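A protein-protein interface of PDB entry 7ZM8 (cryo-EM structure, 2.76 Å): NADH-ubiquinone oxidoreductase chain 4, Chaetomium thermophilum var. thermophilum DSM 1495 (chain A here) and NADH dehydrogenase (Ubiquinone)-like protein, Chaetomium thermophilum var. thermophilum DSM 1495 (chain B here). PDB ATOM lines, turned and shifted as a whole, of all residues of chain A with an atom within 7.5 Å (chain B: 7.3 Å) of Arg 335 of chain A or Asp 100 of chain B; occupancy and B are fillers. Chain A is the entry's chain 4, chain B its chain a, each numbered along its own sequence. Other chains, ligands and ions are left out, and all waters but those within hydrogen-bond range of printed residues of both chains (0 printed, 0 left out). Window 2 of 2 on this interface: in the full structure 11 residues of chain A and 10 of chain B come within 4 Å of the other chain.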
ATOM      1  N   ALA A 329       6.930  -0.481 -21.372  1.00  0.00           N
ATOM      2  CA  ALA A 329       7.087  -1.572 -22.351  1.00  0.00           C
ATOM      3  C   ALA A 329       7.674  -0.977 -23.621  1.00  0.00           C
ATOM      4  O   ALA A 329       8.619  -1.566 -24.134  1.00  0.00           O
ATOM      5  CB  ALA A 329       5.760  -2.227 -22.613  1.00  0.00           C
ATOM      6  N   SER A 330       7.165   0.176 -24.054  1.00  0.00           N
ATOM      7  CA  SER A 330       7.609   0.821 -25.316  1.00  0.00           C
ATOM      8  C   SER A 330       9.032   1.371 -25.221  1.00  0.00           C
ATOM      9  O   SER A 330       9.748   1.304 -26.231  1.00  0.00           O
ATOM     10  CB  SER A 330       6.661   1.903 -25.693  1.00  0.00           C
ATOM     11  OG  SER A 330       5.345   1.394 -25.763  1.00  0.00           O
ATOM     12  N   PHE A 331       9.407   1.933 -24.073  1.00  0.00           N
ATOM     13  CA  PHE A 331      10.776   2.420 -23.929  1.00  0.00           C
ATOM     14  C   PHE A 331      11.773   1.274 -23.987  1.00  0.00           C
ATOM     15  O   PHE A 331      12.844   1.402 -24.587  1.00  0.00           O
ATOM     16  CB  PHE A 331      10.941   3.197 -22.622  1.00  0.00           C
ATOM     17  CG  PHE A 331      10.168   4.482 -22.571  1.00  0.00           C
ATOM     18  CD1 PHE A 331       9.529   4.973 -23.694  1.00  0.00           C
ATOM     19  CD2 PHE A 331      10.093   5.208 -21.398  1.00  0.00           C
ATOM     20  CE1 PHE A 331       8.820   6.143 -23.642  1.00  0.00           C
ATOM     21  CE2 PHE A 331       9.388   6.383 -21.344  1.00  0.00           C
ATOM     22  CZ  PHE A 331       8.753   6.854 -22.468  1.00  0.00           C
ATOM     23  N   SER A 332      11.430   0.143 -23.379  1.00  0.00           N
ATOM     24  CA  SER A 332      12.328  -0.998 -23.352  1.00  0.00           C
ATOM     25  C   SER A 332      12.192  -1.888 -24.576  1.00  0.00           C
ATOM     26  O   SER A 332      13.021  -2.781 -24.769  1.00  0.00           O
ATOM     27  CB  SER A 332      12.104  -1.797 -22.067  1.00  0.00           C
ATOM     28  OG  SER A 332      10.736  -1.994 -21.816  1.00  0.00           O
ATOM     29  N   THR A 333      11.183  -1.658 -25.415  1.00  0.00           N
ATOM     30  CA  THR A 333      11.154  -2.312 -26.717  1.00  0.00           C
ATOM     31  C   THR A 333      12.121  -1.637 -27.679  1.00  0.00           C
ATOM     32  O   THR A 333      12.545  -2.246 -28.666  1.00  0.00           O
ATOM     33  CB  THR A 333       9.735  -2.298 -27.287  1.00  0.00           C
ATOM     34  OG1 THR A 333       8.805  -2.644 -26.260  1.00  0.00           O
ATOM     35  CG2 THR A 333       9.592  -3.316 -28.393  1.00  0.00           C
ATOM     36  N   LEU A 334      12.483  -0.384 -27.406  1.00  0.00           N
ATOM     37  CA  LEU A 334      13.427   0.321 -28.264  1.00  0.00           C
ATOM     38  C   LEU A 334      14.847  -0.199 -28.108  1.00  0.00           C
ATOM     39  O   LEU A 334      15.643  -0.098 -29.047  1.00  0.00           O
ATOM     40  CB  LEU A 334      13.391   1.816 -27.971  1.00  0.00           C
ATOM     41  CG  LEU A 334      12.498   2.658 -28.870  1.00  0.00           C
ATOM     42  CD1 LEU A 334      12.418   4.059 -28.316  1.00  0.00           C
ATOM     43  CD2 LEU A 334      13.033   2.668 -30.286  1.00  0.00           C
ATOM     44  N   ARG A 335      15.188  -0.743 -26.942  1.00  0.00           N
ATOM     45  CA  ARG A 335      16.553  -1.145 -26.637  1.00  0.00           C
ATOM     46  C   ARG A 335      16.736  -2.655 -26.589  1.00  0.00           C
ATOM     47  O   ARG A 335      17.756  -3.130 -26.086  1.00  0.00           O
ATOM     48  CB  ARG A 335      16.992  -0.518 -25.316  1.00  0.00           C
ATOM     49  CG  ARG A 335      17.099   0.989 -25.363  1.00  0.00           C
ATOM     50  CD  ARG A 335      18.289   1.455 -26.170  1.00  0.00           C
ATOM     51  NE  ARG A 335      19.550   0.928 -25.669  1.00  0.00           N
ATOM     52  CZ  ARG A 335      20.264   1.495 -24.705  1.00  0.00           C
ATOM     53  NH1 ARG A 335      19.836   2.605 -24.128  1.00  0.00           N
ATOM     54  NH2 ARG A 335      21.402   0.945 -24.312  1.00  0.00           N
ATOM     55  N   THR A 336      15.784  -3.418 -27.109  1.00  0.00           N
ATOM     56  CA  THR A 336      15.888  -4.869 -27.120  1.00  0.00           C
ATOM     57  C   THR A 336      16.735  -5.318 -28.305  1.00  0.00           C
ATOM     58  O   THR A 336      16.540  -4.854 -29.432  1.00  0.00           O
ATOM     59  CB  THR A 336      14.492  -5.492 -27.179  1.00  0.00           C
ATOM     60  OG1 THR A 336      13.781  -5.165 -25.982  1.00  0.00           O
ATOM     61  CG2 THR A 336      14.573  -7.000 -27.300  1.00  0.00           C
ATOM     62  N   VAL A 337      17.670  -6.237 -28.067  1.00  0.00           N
ATOM     63  CA  VAL A 337      18.623  -6.658 -29.134  1.00  0.00           C
ATOM     64  C   VAL A 337      18.280  -8.042 -29.702  1.00  0.00           C
ATOM     65  O   VAL A 337      18.965  -8.448 -30.642  1.00  0.00           O
ATOM     66  CB  VAL A 337      20.053  -6.629 -28.572  1.00  0.00           C
ATOM     67  CG1 VAL A 337      20.307  -5.361 -27.778  1.00  0.00           C
ATOM     68  CG2 VAL A 337      20.350  -7.846 -27.710  1.00  0.00           C
ATOM     69  N   ASP A 338      17.252  -8.717 -29.193  1.00  0.00           N
ATOM     70  CA  ASP A 338      16.795 -10.017 -29.749  1.00  0.00           C
ATOM     71  C   ASP A 338      15.566  -9.701 -30.600  1.00  0.00           C
ATOM     72  O   ASP A 338      14.669  -9.047 -30.073  1.00  0.00           O
ATOM     73  CB  ASP A 338      16.481 -10.972 -28.597  1.00  0.00           C
ATOM     74  CG  ASP A 338      16.119 -12.398 -28.975  1.00  0.00           C
ATOM     75  OD1 ASP A 338      15.215 -12.585 -29.806  1.00  0.00           O
ATOM     76  OD2 ASP A 338      16.731 -13.317 -28.403  1.00  0.00           O
ATOM     77  N   LEU A 342      11.821  -8.597 -29.439  1.00  0.00           N
ATOM     78  CA  LEU A 342      11.280  -7.292 -29.791  1.00  0.00           C
ATOM     79  C   LEU A 342       9.842  -7.421 -30.274  1.00  0.00           C
ATOM     80  O   LEU A 342       9.014  -6.536 -30.036  1.00  0.00           O
ATOM     81  CB  LEU A 342      12.160  -6.647 -30.861  1.00  0.00           C
ATOM     82  CG  LEU A 342      12.047  -5.162 -31.213  1.00  0.00           C
ATOM     83  CD1 LEU A 342      13.375  -4.706 -31.786  1.00  0.00           C
ATOM     84  CD2 LEU A 342      10.914  -4.855 -32.182  1.00  0.00           C
ATOM     85  N   TYR A 401      22.189  -7.333 -34.151  1.00  0.00           N
ATOM     86  CA  TYR A 401      23.526  -6.910 -34.544  1.00  0.00           C
ATOM     87  C   TYR A 401      23.930  -7.487 -35.890  1.00  0.00           C
ATOM     88  O   TYR A 401      24.655  -6.839 -36.649  1.00  0.00           O
ATOM     89  CB  TYR A 401      24.537  -7.336 -33.486  1.00  0.00           C
ATOM     90  CG  TYR A 401      24.286  -6.747 -32.130  1.00  0.00           C
ATOM     91  CD1 TYR A 401      23.993  -5.408 -31.982  1.00  0.00           C
ATOM     92  CD2 TYR A 401      24.356  -7.531 -30.993  1.00  0.00           C
ATOM     93  CE1 TYR A 401      23.767  -4.870 -30.746  1.00  0.00           C
ATOM     94  CE2 TYR A 401      24.128  -6.999 -29.752  1.00  0.00           C
ATOM     95  CZ  TYR A 401      23.837  -5.670 -29.635  1.00  0.00           C
ATOM     96  OH  TYR A 401      23.612  -5.129 -28.394  1.00  0.00           O
ATOM     97  N   TYR A 464       9.623   2.131 -32.496  1.00  0.00           N
ATOM     98  CA  TYR A 464      10.299   0.817 -32.490  1.00  0.00           C
ATOM     99  C   TYR A 464      10.026   0.046 -33.780  1.00  0.00           C
ATOM    100  O   TYR A 464      10.890  -0.733 -34.176  1.00  0.00           O
ATOM    101  CB  TYR A 464      10.045   0.046 -31.186  1.00  0.00           C
ATOM    102  CG  TYR A 464       8.629  -0.287 -30.796  1.00  0.00           C
ATOM    103  CD1 TYR A 464       7.843  -1.123 -31.569  1.00  0.00           C
ATOM    104  CD2 TYR A 464       8.110   0.156 -29.593  1.00  0.00           C
ATOM    105  CE1 TYR A 464       6.554  -1.452 -31.190  1.00  0.00           C
ATOM    106  CE2 TYR A 464       6.825  -0.165 -29.198  1.00  0.00           C
ATOM    107  CZ  TYR A 464       6.044  -0.975 -29.999  1.00  0.00           C
ATOM    108  OH  TYR A 464       4.778  -1.300 -29.614  1.00  0.00           O
ATOM    109  N   TYR A 467      12.230   1.505 -36.540  1.00  0.00           N
ATOM    110  CA  TYR A 467      13.647   1.341 -36.128  1.00  0.00           C
ATOM    111  C   TYR A 467      14.087  -0.102 -36.325  1.00  0.00           C
ATOM    112  O   TYR A 467      15.184  -0.307 -36.848  1.00  0.00           O
ATOM    113  CB  TYR A 467      13.903   1.883 -34.725  1.00  0.00           C
ATOM    114  CG  TYR A 467      15.359   2.006 -34.353  1.00  0.00           C
ATOM    115  CD1 TYR A 467      16.306   2.422 -35.274  1.00  0.00           C
ATOM    116  CD2 TYR A 467      15.790   1.718 -33.071  1.00  0.00           C
ATOM    117  CE1 TYR A 467      17.643   2.534 -34.935  1.00  0.00           C
ATOM    118  CE2 TYR A 467      17.122   1.824 -32.713  1.00  0.00           C
ATOM    119  CZ  TYR A 467      18.053   2.233 -33.648  1.00  0.00           C
ATOM    120  OH  TYR A 467      19.368   2.343 -33.295  1.00  0.00           O
ATOM    121  N   ARG A 471      16.650  -1.399 -39.447  1.00  0.00           N
ATOM    122  CA  ARG A 471      17.898  -2.031 -39.050  1.00  0.00           C
ATOM    123  C   ARG A 471      18.075  -3.407 -39.673  1.00  0.00           C
ATOM    124  O   ARG A 471      19.197  -3.916 -39.718  1.00  0.00           O
ATOM    125  CB  ARG A 471      17.973  -2.121 -37.531  1.00  0.00           C
ATOM    126  CG  ARG A 471      18.650  -0.930 -36.893  1.00  0.00           C
ATOM    127  CD  ARG A 471      18.686  -1.077 -35.402  1.00  0.00           C
ATOM    128  NE  ARG A 471      17.351  -1.228 -34.842  1.00  0.00           N
ATOM    129  CZ  ARG A 471      17.114  -1.631 -33.603  1.00  0.00           C
ATOM    130  NH1 ARG A 471      15.873  -1.742 -33.168  1.00  0.00           N
ATOM    131  NH2 ARG A 471      18.124  -1.933 -32.804  1.00  0.00           N
ATOM    132  N   TYR B  67      31.511  -8.250 -17.012  1.00  0.00           N
ATOM    133  CA  TYR B  67      31.798  -7.932 -18.402  1.00  0.00           C
ATOM    134  C   TYR B  67      32.689  -6.705 -18.497  1.00  0.00           C
ATOM    135  O   TYR B  67      32.343  -5.635 -17.990  1.00  0.00           O
ATOM    136  CB  TYR B  67      30.479  -7.703 -19.141  1.00  0.00           C
ATOM    137  CG  TYR B  67      30.591  -7.406 -20.615  1.00  0.00           C
ATOM    138  CD1 TYR B  67      30.612  -8.429 -21.548  1.00  0.00           C
ATOM    139  CD2 TYR B  67      30.647  -6.102 -21.076  1.00  0.00           C
ATOM    140  CE1 TYR B  67      30.701  -8.161 -22.898  1.00  0.00           C
ATOM    141  CE2 TYR B  67      30.732  -5.825 -22.416  1.00  0.00           C
ATOM    142  CZ  TYR B  67      30.759  -6.856 -23.326  1.00  0.00           C
ATOM    143  OH  TYR B  67      30.848  -6.577 -24.667  1.00  0.00           O
ATOM    144  N   ASN B  69      34.249  -3.578 -20.285  1.00  0.00           N
ATOM    145  CA  ASN B  69      33.511  -2.673 -21.150  1.00  0.00           C
ATOM    146  C   ASN B  69      34.457  -1.676 -21.801  1.00  0.00           C
ATOM    147  O   ASN B  69      35.226  -1.008 -21.092  1.00  0.00           O
ATOM    148  CB  ASN B  69      32.442  -1.945 -20.337  1.00  0.00           C
ATOM    149  CG  ASN B  69      31.174  -1.736 -21.108  1.00  0.00           C
ATOM    150  OD1 ASN B  69      31.081  -2.093 -22.276  1.00  0.00           O
ATOM    151  ND2 ASN B  69      30.171  -1.176 -20.452  1.00  0.00           N
ATOM    152  N   ARG B  72      32.599   4.142 -23.876  1.00  0.00           N
ATOM    153  CA  ARG B  72      31.313   4.370 -24.526  1.00  0.00           C
ATOM    154  C   ARG B  72      31.473   5.536 -25.488  1.00  0.00           C
ATOM    155  O   ARG B  72      31.137   6.680 -25.181  1.00  0.00           O
ATOM    156  CB  ARG B  72      30.228   4.640 -23.494  1.00  0.00           C
ATOM    157  CG  ARG B  72      28.850   4.659 -24.083  1.00  0.00           C
ATOM    158  CD  ARG B  72      27.790   4.826 -23.036  1.00  0.00           C
ATOM    159  NE  ARG B  72      26.487   5.052 -23.650  1.00  0.00           N
ATOM    160  CZ  ARG B  72      26.139   6.168 -24.281  1.00  0.00           C
ATOM    161  NH1 ARG B  72      24.930   6.274 -24.813  1.00  0.00           N
ATOM    162  NH2 ARG B  72      26.988   7.183 -24.372  1.00  0.00           N
ATOM    163  N   LYS B  74      30.793   6.972 -29.451  1.00  0.00           N
ATOM    164  CA  LYS B  74      30.071   6.830 -30.704  1.00  0.00           C
ATOM    165  C   LYS B  74      31.043   6.579 -31.843  1.00  0.00           C
ATOM    166  O   LYS B  74      32.089   7.223 -31.942  1.00  0.00           O
ATOM    167  CB  LYS B  74      29.251   8.085 -30.989  1.00  0.00           C
ATOM    168  CG  LYS B  74      28.107   8.300 -30.035  1.00  0.00           C
ATOM    169  CD  LYS B  74      26.913   7.476 -30.433  1.00  0.00           C
ATOM    170  CE  LYS B  74      25.800   8.371 -30.935  1.00  0.00           C
ATOM    171  NZ  LYS B  74      24.576   7.594 -31.246  1.00  0.00           N
ATOM    172  N   ARG B  75      30.685   5.654 -32.722  1.00  0.00           N
ATOM    173  CA  ARG B  75      31.595   5.296 -33.796  1.00  0.00           C
ATOM    174  C   ARG B  75      31.652   6.340 -34.897  1.00  0.00           C
ATOM    175  O   ARG B  75      32.445   6.184 -35.826  1.00  0.00           O
ATOM    176  CB  ARG B  75      31.217   3.927 -34.360  1.00  0.00           C
ATOM    177  CG  ARG B  75      31.874   2.799 -33.596  1.00  0.00           C
ATOM    178  CD  ARG B  75      31.415   1.442 -34.042  1.00  0.00           C
ATOM    179  NE  ARG B  75      30.361   0.937 -33.172  1.00  0.00           N
ATOM    180  CZ  ARG B  75      29.223   0.408 -33.604  1.00  0.00           C
ATOM    181  NH1 ARG B  75      28.321  -0.014 -32.735  1.00  0.00           N
ATOM    182  NH2 ARG B  75      28.993   0.296 -34.903  1.00  0.00           N
ATOM    183  N   VAL B  97      33.019  -4.806 -27.894  1.00  0.00           N
ATOM    184  CA  VAL B  97      31.868  -3.931 -28.053  1.00  0.00           C
ATOM    185  C   VAL B  97      31.408  -3.466 -26.681  1.00  0.00           C
ATOM    186  O   VAL B  97      31.364  -4.253 -25.731  1.00  0.00           O
ATOM    187  CB  VAL B  97      30.725  -4.638 -28.812  1.00  0.00           C
ATOM    188  CG1 VAL B  97      31.099  -4.811 -30.267  1.00  0.00           C
ATOM    189  CG2 VAL B  97      30.432  -5.980 -28.198  1.00  0.00           C
ATOM    190  N   HIS B  98      31.093  -2.180 -26.574  1.00  0.00           N
ATOM    191  CA  HIS B  98      30.434  -1.680 -25.379  1.00  0.00           C
ATOM    192  C   HIS B  98      29.042  -2.288 -25.273  1.00  0.00           C
ATOM    193  O   HIS B  98      28.409  -2.621 -26.275  1.00  0.00           O
ATOM    194  CB  HIS B  98      30.353  -0.153 -25.415  1.00  0.00           C
ATOM    195  CG  HIS B  98      29.946   0.472 -24.117  1.00  0.00           C
ATOM    196  ND1 HIS B  98      28.630   0.608 -23.735  1.00  0.00           N
ATOM    197  CD2 HIS B  98      30.682   1.014 -23.120  1.00  0.00           C
ATOM    198  CE1 HIS B  98      28.573   1.191 -22.552  1.00  0.00           C
ATOM    199  NE2 HIS B  98      29.805   1.453 -22.159  1.00  0.00           N
ATOM    200  N   GLU B  99      28.562  -2.434 -24.040  1.00  0.00           N
ATOM    201  CA  GLU B  99      27.251  -3.035 -23.828  1.00  0.00           C
ATOM    202  C   GLU B  99      26.132  -2.212 -24.447  1.00  0.00           C
ATOM    203  O   GLU B  99      25.016  -2.718 -24.598  1.00  0.00           O
ATOM    204  CB  GLU B  99      26.994  -3.215 -22.338  1.00  0.00           C
ATOM    205  CG  GLU B  99      26.890  -1.916 -21.578  1.00  0.00           C
ATOM    206  CD  GLU B  99      26.700  -2.130 -20.095  1.00  0.00           C
ATOM    207  OE1 GLU B  99      26.673  -3.301 -19.660  1.00  0.00           O
ATOM    208  OE2 GLU B  99      26.574  -1.127 -19.361  1.00  0.00           O
ATOM    209  N   ASP B 100      26.406  -0.962 -24.810  1.00  0.00           N
ATOM    210  CA  ASP B 100      25.431  -0.060 -25.414  1.00  0.00           C
ATOM    211  C   ASP B 100      25.569  -0.026 -26.927  1.00  0.00           C
ATOM    212  O   ASP B 100      25.334   1.001 -27.559  1.00  0.00           O
ATOM    213  CB  ASP B 100      25.581   1.337 -24.828  1.00  0.00           C
ATOM    214  CG  ASP B 100      24.851   1.492 -23.518  1.00  0.00           C
ATOM    215  OD1 ASP B 100      24.621   0.473 -22.844  1.00  0.00           O
ATOM    216  OD2 ASP B 100      24.507   2.635 -23.160  1.00  0.00           O
ATOM    217  N   HIS B 101      26.051  -1.124 -27.504  1.00  0.00           N
ATOM    218  CA  HIS B 101      26.324  -1.208 -28.964  1.00  0.00           C
ATOM    219  C   HIS B 101      25.183  -0.638 -29.817  1.00  0.00           C
ATOM    220  O   HIS B 101      25.500   0.001 -30.834  1.00  0.00           O
ATOM    221  CB  HIS B 101      26.675  -2.668 -29.296  1.00  0.00           C
ATOM    222  CG  HIS B 101      27.271  -2.905 -30.641  1.00  0.00           C
ATOM    223  ND1 HIS B 101      28.598  -2.658 -30.914  1.00  0.00           N
ATOM    224  CD2 HIS B 101      26.742  -3.405 -31.777  1.00  0.00           C
ATOM    225  CE1 HIS B 101      28.857  -2.982 -32.163  1.00  0.00           C
ATOM    226  NE2 HIS B 101      27.735  -3.439 -32.713  1.00  0.00           N
ATOM    227  N   ASP B 102      23.919  -0.856 -29.433  1.00  0.00           N
ATOM    228  CA  ASP B 102      22.804  -0.430 -30.275  1.00  0.00           C
ATOM    229  C   ASP B 102      22.902   1.045 -30.622  1.00  0.00           C
ATOM    230  O   ASP B 102      22.829   1.430 -31.794  1.00  0.00           O
ATOM    231  CB  ASP B 102      21.478  -0.693 -29.564  1.00  0.00           C
ATOM    232  CG  ASP B 102      21.396  -2.074 -28.974  1.00  0.00           C
ATOM    233  OD1 ASP B 102      21.668  -3.043 -29.704  1.00  0.00           O
ATOM    234  OD2 ASP B 102      21.061  -2.188 -27.776  1.00  0.00           O
ATOM    235  N   ILE B 103      23.061   1.889 -29.613  1.00  0.00           N
ATOM    236  CA  ILE B 103      22.963   3.324 -29.788  1.00  0.00           C
ATOM    237  C   ILE B 103      24.342   3.981 -29.826  1.00  0.00           C
ATOM    238  O   ILE B 103      24.474   5.160 -29.511  1.00  0.00           O
ATOM    239  CB  ILE B 103      22.064   3.952 -28.715  1.00  0.00           C
ATOM    240  CG1 ILE B 103      22.558   3.594 -27.318  1.00  0.00           C
ATOM    241  CG2 ILE B 103      20.658   3.445 -28.878  1.00  0.00           C
ATOM    242  CD1 ILE B 103      21.833   4.341 -26.230  1.00  0.00           C
ATOM    243  N   LEU B 104      25.371   3.227 -30.198  1.00  0.00           N
ATOM    244  CA  LEU B 104      26.709   3.759 -30.379  1.00  0.00           C
ATOM    245  C   LEU B 104      27.190   3.645 -31.816  1.00  0.00           C
ATOM    246  O   LEU B 104      28.296   4.100 -32.120  1.00  0.00           O
ATOM    247  CB  LEU B 104      27.701   3.040 -29.458  1.00  0.00           C
ATOM    248  CG  LEU B 104      27.714   3.309 -27.956  1.00  0.00           C
ATOM    249  CD1 LEU B 104      28.747   2.407 -27.310  1.00  0.00           C
ATOM    250  CD2 LEU B 104      27.997   4.765 -27.641  1.00  0.00           C
ATOM    251  N   GLY B 105      26.395   3.046 -32.704  1.00  0.00           N
ATOM    252  CA  GLY B 105      26.815   2.794 -34.063  1.00  0.00           C
ATOM    253  C   GLY B 105      26.475   3.921 -35.013  1.00  0.00           C
ATOM    254  O   GLY B 105      25.960   4.969 -34.634  1.00  0.00           O
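The side-chain carboxylate (OD1) of Asp 100 of chain B is in salt-bridge range of the guanidinium group (NH2) of Arg 335 of chain A. The side-chain hydroxyl (OH) of Tyr 401 of chain A sits close to the side-chain carboxylate (OD1) of Asp 102 of chain B (3.1 Å).
The side-chain carboxylate of Asp 100 of chain B lies within salt-bridge range of the guanidinium group of Arg 72 of chain B, 3.2 Å away. The side-chain amino group (NZ) of Lys 74 of chain B lies within hydrogen-bond range of the backbone carbonyl oxygen (O) of Ile 103 of chain B, at 3.0 Å. A ring nitrogen (ND1) of His 101 of chain B sits close to the guanidinium group (NH1) of Arg 75 of chain B, at 3.2 Å. ND1 of His 98 of chain B is in hydrogen-bond range of N of Asp 100 of chain B (2.9 Å). The backbone carbonyl oxygen of Tyr 467 of chain A is in hydrogen-bond range of the guanidinium group of Arg 471 of chain A (3.1 Å).
Among the printed residues, merely in contact across the chains: Arg 335 of chain A with Asp 102 of chain B, Arg 335 of chain A with Ile 103 of chain B, Val 337 of chain A with Asp 102 of chain B, Tyr 401 of chain A with His 101 of chain B and Tyr 467 of chain A with Asp 102 of chain B.
Phe 331 of chain A touches none of the printed residues of chain B. Arg 335 of chain A touches just these residues of chain B: Asp 100 (3.6 Å), Asp 102 (3.8 Å) and Ile 103 (3.4 Å). Printed residues of chain B within 4 Å of Val 337 of chain A: Asp 102. Of the printed residues of chain B, Tyr 401 of chain A touches His 101 (3.4 Å) and Asp 102 (3.0 Å). Printed residues of chain B within 4 Å of Tyr 467 of chain A: Asp 102. Glu 99 of chain B touches none of the printed residues of chain A. Of chain A, only Arg 335 comes within 4 Å of Asp 100 of chain B. Of the printed residues of chain A, His 101 of chain B touches Tyr 401. Of the printed residues of chain A, Asp 102 of chain B touches Arg 335, Val 337, Tyr 401 and Tyr 467. The nearest residue of chain B that does not touch Arg 335 of chain A is Glu 99 of chain B (5.2 Å). The nearest residue of chain A that does not touch Asp 100 of chain B is Tyr 401 of chain A (5.7 Å).
Of the 15 printed residues of chain A, 4 touch a printed residue of chain B. Printed residues of chain A that touch a printed residue of chain B: Arg 335, Val 337, Tyr 401 and Tyr 467. Of the 14 printed residues of chain B, 4 touch a printed residue of chain A. Hydrophobic or aromatic side chains of chain B within 4 Å of the printed part of chain A: His 101 and Ile 103. Among the printed residues, 7 pairs touch across the chains. Among the printed residues, Asp or Glu carboxylates within 4 Å of a Lys or Arg side-chain nitrogen of the other chain: Arg 335 of chain A with Asp 100 of chain B (3.6 Å).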
